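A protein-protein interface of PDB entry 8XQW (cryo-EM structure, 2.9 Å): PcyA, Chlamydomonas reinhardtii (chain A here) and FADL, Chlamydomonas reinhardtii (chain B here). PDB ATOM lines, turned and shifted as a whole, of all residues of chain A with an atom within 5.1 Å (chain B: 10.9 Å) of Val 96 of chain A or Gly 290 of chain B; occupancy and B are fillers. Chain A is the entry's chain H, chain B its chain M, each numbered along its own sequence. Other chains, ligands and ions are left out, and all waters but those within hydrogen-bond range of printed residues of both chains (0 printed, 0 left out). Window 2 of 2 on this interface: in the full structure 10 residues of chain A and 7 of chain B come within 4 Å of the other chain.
Pro 288 of chain B touches Ile 92 of chain A. Met 93 of chain A touches Pro 288 of chain B. CD1 of Leu 95 of chain A touches NE2 of Gln 298 of chain B, 3.3 Å away. Val 96 of chain A touches Gly 290 of chain B (CG2 to O, 3.7 Å). CG2 of Val 96 of chain A touches CD1 of Leu 295 of chain B (3.6 Å). Leu 295 of chain B touches His 99 of chain A.
The backbone NH (N) of Gly 290 of chain B sits at hydrogen-bond distance from the side-chain carboxylate (OD2) of Asp 543 of chain B (2.5 Å).
Among the printed residues, 6 pairs touch across the chains. Among the printed residues, no Asp or Glu carboxylate lies within 4 Å of a Lys or Arg side-chain nitrogen of the other chain.
Of the printed residues of chain B, Ile 92 of chain A touches Pro 288 (3.6 Å). Printed residues of chain B within 4 Å of Met 93 of chain A: Pro 288 (3.4 Å). Leu 95 of chain A touches one residue of chain B. Printed residues of chain B within 4 Å of Val 96 of chain A: Gly 290 and Leu 295. Of chain B, only Leu 295 (3.9 Å) comes within 4 Å of His 99 of chain A. No residue of chain B comes within 4 Å of Glu 100 of chain A. Printed residues of chain A within 4 Å of Pro 288 of chain B: Ile 92 (3.6 Å) and Met 93 (3.4 Å). Gly 290 of chain B touches just one residue of chain A: Val 96 (3.7 Å). Printed residues of chain A within 4 Å of Leu 295 of chain B: Val 96 (3.6 Å) and His 99 (3.9 Å). Printed residues of chain A within 4 Å of Gln 298 of chain B: Leu 95 (3.3 Å). The nearest residue of chain B that does not touch Val 96 of chain A is Ser 291 of chain B (4.1 Å). The nearest printed residue of chain A that does not touch Gly 290 of chain B is Met 93 of chain A (5.7 Å).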
ATOM      1  N   ILE A  92     -14.790 -11.739  -7.401  1.00  0.00           N
ATOM      2  CA  ILE A  92     -13.654 -11.018  -7.956  1.00  0.00           C
ATOM      3  C   ILE A  92     -12.361 -11.536  -7.340  1.00  0.00           C
ATOM      4  O   ILE A  92     -11.374 -11.791  -8.044  1.00  0.00           O
ATOM      5  CB  ILE A  92     -13.827  -9.507  -7.727  1.00  0.00           C
ATOM      6  CG1 ILE A  92     -15.133  -9.020  -8.346  1.00  0.00           C
ATOM      7  CG2 ILE A  92     -12.666  -8.742  -8.313  1.00  0.00           C
ATOM      8  CD1 ILE A  92     -15.305  -9.428  -9.779  1.00  0.00           C
ATOM      9  N   MET A  93     -12.353 -11.717  -6.019  1.00  0.00           N
ATOM     10  CA  MET A  93     -11.167 -12.252  -5.364  1.00  0.00           C
ATOM     11  C   MET A  93     -10.897 -13.683  -5.804  1.00  0.00           C
ATOM     12  O   MET A  93      -9.737 -14.093  -5.925  1.00  0.00           O
ATOM     13  CB  MET A  93     -11.323 -12.174  -3.851  1.00  0.00           C
ATOM     14  CG  MET A  93     -11.278 -10.762  -3.320  1.00  0.00           C
ATOM     15  SD  MET A  93     -12.906 -10.002  -3.329  1.00  0.00           S
ATOM     16  CE  MET A  93     -13.440 -10.328  -1.654  1.00  0.00           C
ATOM     17  N   ARG A  94     -11.951 -14.459  -6.043  1.00  0.00           N
ATOM     18  CA  ARG A  94     -11.767 -15.794  -6.594  1.00  0.00           C
ATOM     19  C   ARG A  94     -11.058 -15.728  -7.936  1.00  0.00           C
ATOM     20  O   ARG A  94     -10.162 -16.531  -8.223  1.00  0.00           O
ATOM     21  CB  ARG A  94     -13.119 -16.485  -6.729  1.00  0.00           C
ATOM     22  CG  ARG A  94     -13.032 -17.946  -7.100  1.00  0.00           C
ATOM     23  CD  ARG A  94     -14.393 -18.489  -7.492  1.00  0.00           C
ATOM     24  NE  ARG A  94     -15.480 -17.638  -7.014  1.00  0.00           N
ATOM     25  CZ  ARG A  94     -16.044 -17.745  -5.815  1.00  0.00           C
ATOM     26  NH1 ARG A  94     -15.615 -18.661  -4.958  1.00  0.00           N
ATOM     27  NH2 ARG A  94     -17.029 -16.930  -5.466  1.00  0.00           N
ATOM     28  N   LEU A  95     -11.445 -14.764  -8.771  1.00  0.00           N
ATOM     29  CA  LEU A  95     -10.793 -14.599 -10.064  1.00  0.00           C
ATOM     30  C   LEU A  95      -9.327 -14.232  -9.897  1.00  0.00           C
ATOM     31  O   LEU A  95      -8.461 -14.761 -10.603  1.00  0.00           O
ATOM     32  CB  LEU A  95     -11.520 -13.537 -10.880  1.00  0.00           C
ATOM     33  CG  LEU A  95     -12.726 -14.026 -11.672  1.00  0.00           C
ATOM     34  CD1 LEU A  95     -13.232 -12.928 -12.578  1.00  0.00           C
ATOM     35  CD2 LEU A  95     -12.359 -15.254 -12.469  1.00  0.00           C
ATOM     36  N   VAL A  96      -9.033 -13.332  -8.959  1.00  0.00           N
ATOM     37  CA  VAL A  96      -7.645 -12.947  -8.712  1.00  0.00           C
ATOM     38  C   VAL A  96      -6.825 -14.159  -8.298  1.00  0.00           C
ATOM     39  O   VAL A  96      -5.716 -14.388  -8.806  1.00  0.00           O
ATOM     40  CB  VAL A  96      -7.584 -11.852  -7.635  1.00  0.00           C
ATOM     41  CG1 VAL A  96      -6.154 -11.608  -7.220  1.00  0.00           C
ATOM     42  CG2 VAL A  96      -8.211 -10.579  -8.133  1.00  0.00           C
ATOM     43  N   GLN A  97      -7.362 -14.954  -7.373  1.00  0.00           N
ATOM     44  CA  GLN A  97      -6.648 -16.129  -6.897  1.00  0.00           C
ATOM     45  C   GLN A  97      -6.376 -17.090  -8.038  1.00  0.00           C
ATOM     46  O   GLN A  97      -5.244 -17.552  -8.224  1.00  0.00           O
ATOM     47  CB  GLN A  97      -7.449 -16.820  -5.800  1.00  0.00           C
ATOM     48  CG  GLN A  97      -7.473 -16.058  -4.501  1.00  0.00           C
ATOM     49  CD  GLN A  97      -6.104 -15.943  -3.883  1.00  0.00           C
ATOM     50  OE1 GLN A  97      -5.242 -16.795  -4.094  1.00  0.00           O
ATOM     51  NE2 GLN A  97      -5.890 -14.884  -3.116  1.00  0.00           N
ATOM     52  N   GLN A  98      -7.409 -17.411  -8.811  1.00  0.00           N
ATOM     53  CA  GLN A  98      -7.242 -18.364  -9.896  1.00  0.00           C
ATOM     54  C   GLN A  98      -6.215 -17.876 -10.904  1.00  0.00           C
ATOM     55  O   GLN A  98      -5.401 -18.661 -11.406  1.00  0.00           O
ATOM     56  CB  GLN A  98      -8.588 -18.617 -10.563  1.00  0.00           C
ATOM     57  CG  GLN A  98      -8.505 -18.963 -12.022  1.00  0.00           C
ATOM     58  CD  GLN A  98      -9.863 -19.264 -12.604  1.00  0.00           C
ATOM     59  OE1 GLN A  98     -10.145 -18.940 -13.757  1.00  0.00           O
ATOM     60  NE2 GLN A  98     -10.721 -19.884 -11.804  1.00  0.00           N
ATOM     61  N   HIS A  99      -6.210 -16.575 -11.187  1.00  0.00           N
ATOM     62  CA  HIS A  99      -5.262 -16.048 -12.161  1.00  0.00           C
ATOM     63  C   HIS A  99      -3.828 -16.181 -11.670  1.00  0.00           C
ATOM     64  O   HIS A  99      -2.951 -16.672 -12.396  1.00  0.00           O
ATOM     65  CB  HIS A  99      -5.583 -14.594 -12.472  1.00  0.00           C
ATOM     66  CG  HIS A  99      -4.593 -13.953 -13.384  1.00  0.00           C
ATOM     67  ND1 HIS A  99      -4.146 -14.560 -14.535  1.00  0.00           N
ATOM     68  CD2 HIS A  99      -3.954 -12.761 -13.312  1.00  0.00           C
ATOM     69  CE1 HIS A  99      -3.277 -13.769 -15.137  1.00  0.00           C
ATOM     70  NE2 HIS A  99      -3.142 -12.672 -14.415  1.00  0.00           N
ATOM     71  N   GLU A 100      -3.559 -15.741 -10.441  1.00  0.00           N
ATOM     72  CA  GLU A 100      -2.180 -15.836  -9.972  1.00  0.00           C
ATOM     73  C   GLU A 100      -1.747 -17.286  -9.805  1.00  0.00           C
ATOM     74  O   GLU A 100      -0.569 -17.611 -10.015  1.00  0.00           O
ATOM     75  CB  GLU A 100      -1.990 -15.054  -8.676  1.00  0.00           C
ATOM     76  CG  GLU A 100      -2.816 -15.523  -7.514  1.00  0.00           C
ATOM     77  CD  GLU A 100      -2.906 -14.473  -6.431  1.00  0.00           C
ATOM     78  OE1 GLU A 100      -2.410 -13.349  -6.652  1.00  0.00           O
ATOM     79  OE2 GLU A 100      -3.475 -14.765  -5.359  1.00  0.00           O
ATOM     80  N   ASP A 101      -2.681 -18.179  -9.475  1.00  0.00           N
ATOM     81  CA  ASP A 101      -2.339 -19.591  -9.370  1.00  0.00           C
ATOM     82  C   ASP A 101      -1.946 -20.165 -10.721  1.00  0.00           C
ATOM     83  O   ASP A 101      -0.958 -20.900 -10.828  1.00  0.00           O
ATOM     84  CB  ASP A 101      -3.507 -20.370  -8.776  1.00  0.00           C
ATOM     85  CG  ASP A 101      -3.723 -20.053  -7.319  1.00  0.00           C
ATOM     86  OD1 ASP A 101      -3.212 -19.009  -6.867  1.00  0.00           O
ATOM     87  OD2 ASP A 101      -4.399 -20.843  -6.627  1.00  0.00           O
ATOM     88  N   ASP B 286     -19.422  -0.705  -4.666  1.00  0.00           N
ATOM     89  CA  ASP B 286     -18.033  -0.722  -4.127  1.00  0.00           C
ATOM     90  C   ASP B 286     -17.287  -1.956  -4.635  1.00  0.00           C
ATOM     91  O   ASP B 286     -17.821  -3.076  -4.507  1.00  0.00           O
ATOM     92  CB  ASP B 286     -18.019  -0.552  -2.617  1.00  0.00           C
ATOM     93  CG  ASP B 286     -18.054   0.896  -2.160  1.00  0.00           C
ATOM     94  OD1 ASP B 286     -19.136   1.505  -2.247  1.00  0.00           O
ATOM     95  OD2 ASP B 286     -16.995   1.406  -1.749  1.00  0.00           O
ATOM     96  N   PHE B 287     -16.092  -1.744  -5.180  1.00  0.00           N
ATOM     97  CA  PHE B 287     -15.314  -2.860  -5.761  1.00  0.00           C
ATOM     98  C   PHE B 287     -14.337  -3.368  -4.717  1.00  0.00           C
ATOM     99  O   PHE B 287     -13.815  -2.568  -3.920  1.00  0.00           O
ATOM    100  CB  PHE B 287     -14.730  -2.185  -7.002  1.00  0.00           C
ATOM    101  CG  PHE B 287     -14.031  -3.087  -8.000  1.00  0.00           C
ATOM    102  CD1 PHE B 287     -14.755  -3.774  -8.961  1.00  0.00           C
ATOM    103  CD2 PHE B 287     -12.652  -3.221  -7.979  1.00  0.00           C
ATOM    104  CE1 PHE B 287     -14.109  -4.586  -9.871  1.00  0.00           C
ATOM    105  CE2 PHE B 287     -12.013  -4.037  -8.890  1.00  0.00           C
ATOM    106  CZ  PHE B 287     -12.742  -4.713  -9.830  1.00  0.00           C
ATOM    107  N   PRO B 288     -14.064  -4.686  -4.670  1.00  0.00           N
ATOM    108  CA  PRO B 288     -13.072  -5.217  -3.750  1.00  0.00           C
ATOM    109  C   PRO B 288     -11.674  -4.697  -4.030  1.00  0.00           C
ATOM    110  O   PRO B 288     -11.355  -4.390  -5.188  1.00  0.00           O
ATOM    111  CB  PRO B 288     -13.177  -6.694  -4.074  1.00  0.00           C
ATOM    112  CG  PRO B 288     -13.619  -6.728  -5.506  1.00  0.00           C
ATOM    113  CD  PRO B 288     -14.703  -5.683  -5.500  1.00  0.00           C
ATOM    114  N   PRO B 289     -10.784  -4.597  -3.023  1.00  0.00           N
ATOM    115  CA  PRO B 289      -9.413  -4.181  -3.278  1.00  0.00           C
ATOM    116  C   PRO B 289      -8.523  -5.272  -3.850  1.00  0.00           C
ATOM    117  O   PRO B 289      -9.017  -6.396  -4.046  1.00  0.00           O
ATOM    118  CB  PRO B 289      -8.994  -3.804  -1.862  1.00  0.00           C
ATOM    119  CG  PRO B 289      -9.716  -4.796  -0.997  1.00  0.00           C
ATOM    120  CD  PRO B 289     -11.088  -4.850  -1.631  1.00  0.00           C
ATOM    121  N   GLY B 290      -7.250  -4.967  -4.137  1.00  0.00           N
ATOM    122  CA  GLY B 290      -6.353  -6.021  -4.562  1.00  0.00           C
ATOM    123  C   GLY B 290      -6.760  -6.680  -5.859  1.00  0.00           C
ATOM    124  O   GLY B 290      -7.135  -7.855  -5.874  1.00  0.00           O
ATOM    125  N   SER B 291      -6.697  -5.937  -6.957  1.00  0.00           N
ATOM    126  CA  SER B 291      -7.053  -6.469  -8.260  1.00  0.00           C
ATOM    127  C   SER B 291      -6.247  -5.729  -9.313  1.00  0.00           C
ATOM    128  O   SER B 291      -5.305  -4.996  -8.999  1.00  0.00           O
ATOM    129  CB  SER B 291      -8.560  -6.346  -8.508  1.00  0.00           C
ATOM    130  OG  SER B 291      -8.895  -6.841  -9.790  1.00  0.00           O
ATOM    131  N   HIS B 292      -6.619  -5.921 -10.574  1.00  0.00           N
ATOM    132  CA  HIS B 292      -5.983  -5.208 -11.648  1.00  0.00           C
ATOM    133  C   HIS B 292      -6.950  -5.155 -12.816  1.00  0.00           C
ATOM    134  O   HIS B 292      -7.697  -6.119 -13.032  1.00  0.00           O
ATOM    135  CB  HIS B 292      -4.679  -5.865 -12.081  1.00  0.00           C
ATOM    136  CG  HIS B 292      -3.722  -4.919 -12.723  1.00  0.00           C
ATOM    137  ND1 HIS B 292      -3.524  -4.871 -14.084  1.00  0.00           N
ATOM    138  CD2 HIS B 292      -2.918  -3.967 -12.193  1.00  0.00           C
ATOM    139  CE1 HIS B 292      -2.634  -3.937 -14.366  1.00  0.00           C
ATOM    140  NE2 HIS B 292      -2.251  -3.375 -13.235  1.00  0.00           N
ATOM    141  N   PRO B 293      -6.970  -4.060 -13.570  1.00  0.00           N
ATOM    142  CA  PRO B 293      -7.909  -3.964 -14.692  1.00  0.00           C
ATOM    143  C   PRO B 293      -7.710  -5.030 -15.739  1.00  0.00           C
ATOM    144  O   PRO B 293      -8.697  -5.525 -16.286  1.00  0.00           O
ATOM    145  CB  PRO B 293      -7.628  -2.571 -15.261  1.00  0.00           C
ATOM    146  CG  PRO B 293      -7.008  -1.836 -14.154  1.00  0.00           C
ATOM    147  CD  PRO B 293      -6.226  -2.812 -13.364  1.00  0.00           C
ATOM    148  N   SER B 294      -6.475  -5.420 -16.021  1.00  0.00           N
ATOM    149  CA  SER B 294      -6.192  -6.436 -17.023  1.00  0.00           C
ATOM    150  C   SER B 294      -6.833  -7.778 -16.714  1.00  0.00           C
ATOM    151  O   SER B 294      -6.764  -8.683 -17.550  1.00  0.00           O
ATOM    152  CB  SER B 294      -4.687  -6.628 -17.156  1.00  0.00           C
ATOM    153  OG  SER B 294      -4.181  -7.326 -16.035  1.00  0.00           O
ATOM    154  N   LEU B 295      -7.432  -7.940 -15.539  1.00  0.00           N
ATOM    155  CA  LEU B 295      -8.138  -9.175 -15.235  1.00  0.00           C
ATOM    156  C   LEU B 295      -9.319  -9.373 -16.165  1.00  0.00           C
ATOM    157  O   LEU B 295      -9.424 -10.399 -16.842  1.00  0.00           O
ATOM    158  CB  LEU B 295      -8.624  -9.163 -13.793  1.00  0.00           C
ATOM    159  CG  LEU B 295      -7.955 -10.128 -12.838  1.00  0.00           C
ATOM    160  CD1 LEU B 295      -8.860 -10.299 -11.657  1.00  0.00           C
ATOM    161  CD2 LEU B 295      -7.723 -11.447 -13.525  1.00  0.00           C
ATOM    162  N   PHE B 296     -10.205  -8.389 -16.221  1.00  0.00           N
ATOM    163  CA  PHE B 296     -11.472  -8.503 -16.921  1.00  0.00           C
ATOM    164  C   PHE B 296     -11.316  -8.599 -18.427  1.00  0.00           C
ATOM    165  O   PHE B 296     -12.325  -8.671 -19.132  1.00  0.00           O
ATOM    166  CB  PHE B 296     -12.354  -7.324 -16.542  1.00  0.00           C
ATOM    167  CG  PHE B 296     -12.369  -7.052 -15.075  1.00  0.00           C
ATOM    168  CD1 PHE B 296     -13.202  -7.762 -14.242  1.00  0.00           C
ATOM    169  CD2 PHE B 296     -11.536  -6.103 -14.523  1.00  0.00           C
ATOM    170  CE1 PHE B 296     -13.215  -7.523 -12.892  1.00  0.00           C
ATOM    171  CE2 PHE B 296     -11.546  -5.859 -13.170  1.00  0.00           C
ATOM    172  CZ  PHE B 296     -12.387  -6.570 -12.356  1.00  0.00           C
ATOM    173  N   GLN B 298     -10.487 -11.188 -19.709  1.00  0.00           N
ATOM    174  CA  GLN B 298     -10.954 -12.542 -19.955  1.00  0.00           C
ATOM    175  C   GLN B 298     -12.464 -12.614 -20.113  1.00  0.00           C
ATOM    176  O   GLN B 298     -12.976 -13.642 -20.566  1.00  0.00           O
ATOM    177  CB  GLN B 298     -10.532 -13.455 -18.812  1.00  0.00           C
ATOM    178  CG  GLN B 298     -11.350 -13.238 -17.564  1.00  0.00           C
ATOM    179  CD  GLN B 298     -10.663 -13.741 -16.322  1.00  0.00           C
ATOM    180  OE1 GLN B 298      -9.532 -14.218 -16.372  1.00  0.00           O
ATOM    181  NE2 GLN B 298     -11.344 -13.636 -15.192  1.00  0.00           N
ATOM    182  N   LEU B 299     -13.185 -11.557 -19.735  1.00  0.00           N
ATOM    183  CA  LEU B 299     -14.630 -11.539 -19.903  1.00  0.00           C
ATOM    184  C   LEU B 299     -15.041 -11.170 -21.318  1.00  0.00           C
ATOM    185  O   LEU B 299     -16.238 -11.103 -21.605  1.00  0.00           O
ATOM    186  CB  LEU B 299     -15.259 -10.555 -18.921  1.00  0.00           C
ATOM    187  CG  LEU B 299     -14.769 -10.620 -17.478  1.00  0.00           C
ATOM    188  CD1 LEU B 299     -15.543  -9.648 -16.623  1.00  0.00           C
ATOM    189  CD2 LEU B 299     -14.914 -12.021 -16.939  1.00  0.00           C
ATOM    190  N   GLY B 541      -4.001   3.503   0.358  1.00  0.00           N
ATOM    191  CA  GLY B 541      -5.189   2.887  -0.184  1.00  0.00           C
ATOM    192  C   GLY B 541      -5.380   3.015  -1.673  1.00  0.00           C
ATOM    193  O   GLY B 541      -6.452   2.662  -2.174  1.00  0.00           O
ATOM    194  N   TRP B 542      -4.388   3.502  -2.405  1.00  0.00           N
ATOM    195  CA  TRP B 542      -4.534   3.531  -3.846  1.00  0.00           C
ATOM    196  C   TRP B 542      -4.529   2.114  -4.399  1.00  0.00           C
ATOM    197  O   TRP B 542      -3.625   1.323  -4.134  1.00  0.00           O
ATOM    198  CB  TRP B 542      -3.420   4.343  -4.493  1.00  0.00           C
ATOM    199  CG  TRP B 542      -3.634   4.517  -5.948  1.00  0.00           C
ATOM    200  CD1 TRP B 542      -4.454   5.412  -6.545  1.00  0.00           C
ATOM    201  CD2 TRP B 542      -3.037   3.755  -6.996  1.00  0.00           C
ATOM    202  NE1 TRP B 542      -4.406   5.264  -7.902  1.00  0.00           N
ATOM    203  CE2 TRP B 542      -3.538   4.252  -8.205  1.00  0.00           C
ATOM    204  CE3 TRP B 542      -2.129   2.699  -7.028  1.00  0.00           C
ATOM    205  CZ2 TRP B 542      -3.163   3.734  -9.431  1.00  0.00           C
ATOM    206  CZ3 TRP B 542      -1.756   2.190  -8.244  1.00  0.00           C
ATOM    207  CH2 TRP B 542      -2.269   2.706  -9.430  1.00  0.00           C
ATOM    208  N   ASP B 543      -5.562   1.794  -5.168  1.00  0.00           N
ATOM    209  CA  ASP B 543      -5.682   0.489  -5.794  1.00  0.00           C
ATOM    210  C   ASP B 543      -5.862   0.684  -7.288  1.00  0.00           C
ATOM    211  O   ASP B 543      -6.570   1.595  -7.715  1.00  0.00           O
ATOM    212  CB  ASP B 543      -6.855  -0.298  -5.215  1.00  0.00           C
ATOM    213  CG  ASP B 543      -6.962  -1.690  -5.789  1.00  0.00           C
ATOM    214  OD1 ASP B 543      -7.148  -1.828  -7.015  1.00  0.00           O
ATOM    215  OD2 ASP B 543      -6.865  -2.655  -5.008  1.00  0.00           O
ATOM    216  N   ALA B 544      -5.234  -0.185  -8.075  1.00  0.00           N
ATOM    217  CA  ALA B 544      -5.231   0.000  -9.522  1.00  0.00           C
ATOM    218  C   ALA B 544      -6.580  -0.342 -10.135  1.00  0.00           C
ATOM    219  O   ALA B 544      -7.194   0.494 -10.806  1.00  0.00           O
ATOM    220  CB  ALA B 544      -4.131  -0.846 -10.155  1.00  0.00           C
ATOM    221  N   GLY B 545      -7.049  -1.570  -9.927  1.00  0.00           N
ATOM    222  CA  GLY B 545      -8.319  -1.968 -10.502  1.00  0.00           C
ATOM    223  C   GLY B 545      -9.479  -1.163  -9.964  1.00  0.00           C
ATOM    224  O   GLY B 545     -10.416  -0.843 -10.700  1.00  0.00           O
ATOM    225  N   ARG B 546      -9.431  -0.817  -8.681  1.00  0.00           N
ATOM    226  CA  ARG B 546     -10.495  -0.021  -8.090  1.00  0.00           C
ATOM    227  C   ARG B 546     -10.577   1.350  -8.738  1.00  0.00           C
ATOM    228  O   ARG B 546     -11.668   1.900  -8.901  1.00  0.00           O
ATOM    229  CB  ARG B 546     -10.265   0.097  -6.589  1.00  0.00           C
ATOM    230  CG  ARG B 546     -11.172   1.066  -5.887  1.00  0.00           C
ATOM    231  CD  ARG B 546     -10.579   1.474  -4.554  1.00  0.00           C
ATOM    232  NE  ARG B 546     -10.374   0.330  -3.675  1.00  0.00           N
ATOM    233  CZ  ARG B 546     -11.287  -0.127  -2.827  1.00  0.00           C
ATOM    234  NH1 ARG B 546     -12.468   0.467  -2.749  1.00  0.00           N
ATOM    235  NH2 ARG B 546     -11.023  -1.172  -2.061  1.00  0.00           N
ATOM    236  N   ALA B 547      -9.435   1.912  -9.127  1.00  0.00           N
ATOM    237  CA  ALA B 547      -9.433   3.240  -9.726  1.00  0.00           C
ATOM    238  C   ALA B 547      -9.738   3.192 -11.214  1.00  0.00           C
ATOM    239  O   ALA B 547     -10.229   4.172 -11.773  1.00  0.00           O
ATOM    240  CB  ALA B 547      -8.089   3.922  -9.496  1.00  0.00           C
ATOM    241  N   ALA B 548      -9.450   2.080 -11.874  1.00  0.00           N
ATOM    242  CA  ALA B 548      -9.710   2.041 -13.305  1.00  0.00           C
ATOM    243  C   ALA B 548     -11.115   1.551 -13.614  1.00  0.00           C
ATOM    244  O   ALA B 548     -11.623   1.792 -14.712  1.00  0.00           O
ATOM    245  CB  ALA B 548      -8.683   1.166 -14.006  1.00  0.00           C
ATOM    246  N   VAL B 549     -11.754   0.848 -12.680  1.00  0.00           N
ATOM    247  CA  VAL B 549     -13.118   0.382 -12.919  1.00  0.00           C
ATOM    248  C   VAL B 549     -14.121   1.268 -12.202  1.00  0.00           C
ATOM    249  O   VAL B 549     -15.037   1.824 -12.818  1.00  0.00           O
ATOM    250  CB  VAL B 549     -13.276  -1.085 -12.491  1.00  0.00           C
ATOM    251  CG1 VAL B 549     -14.738  -1.413 -12.337  1.00  0.00           C
ATOM    252  CG2 VAL B 549     -12.649  -1.992 -13.514  1.00  0.00           C
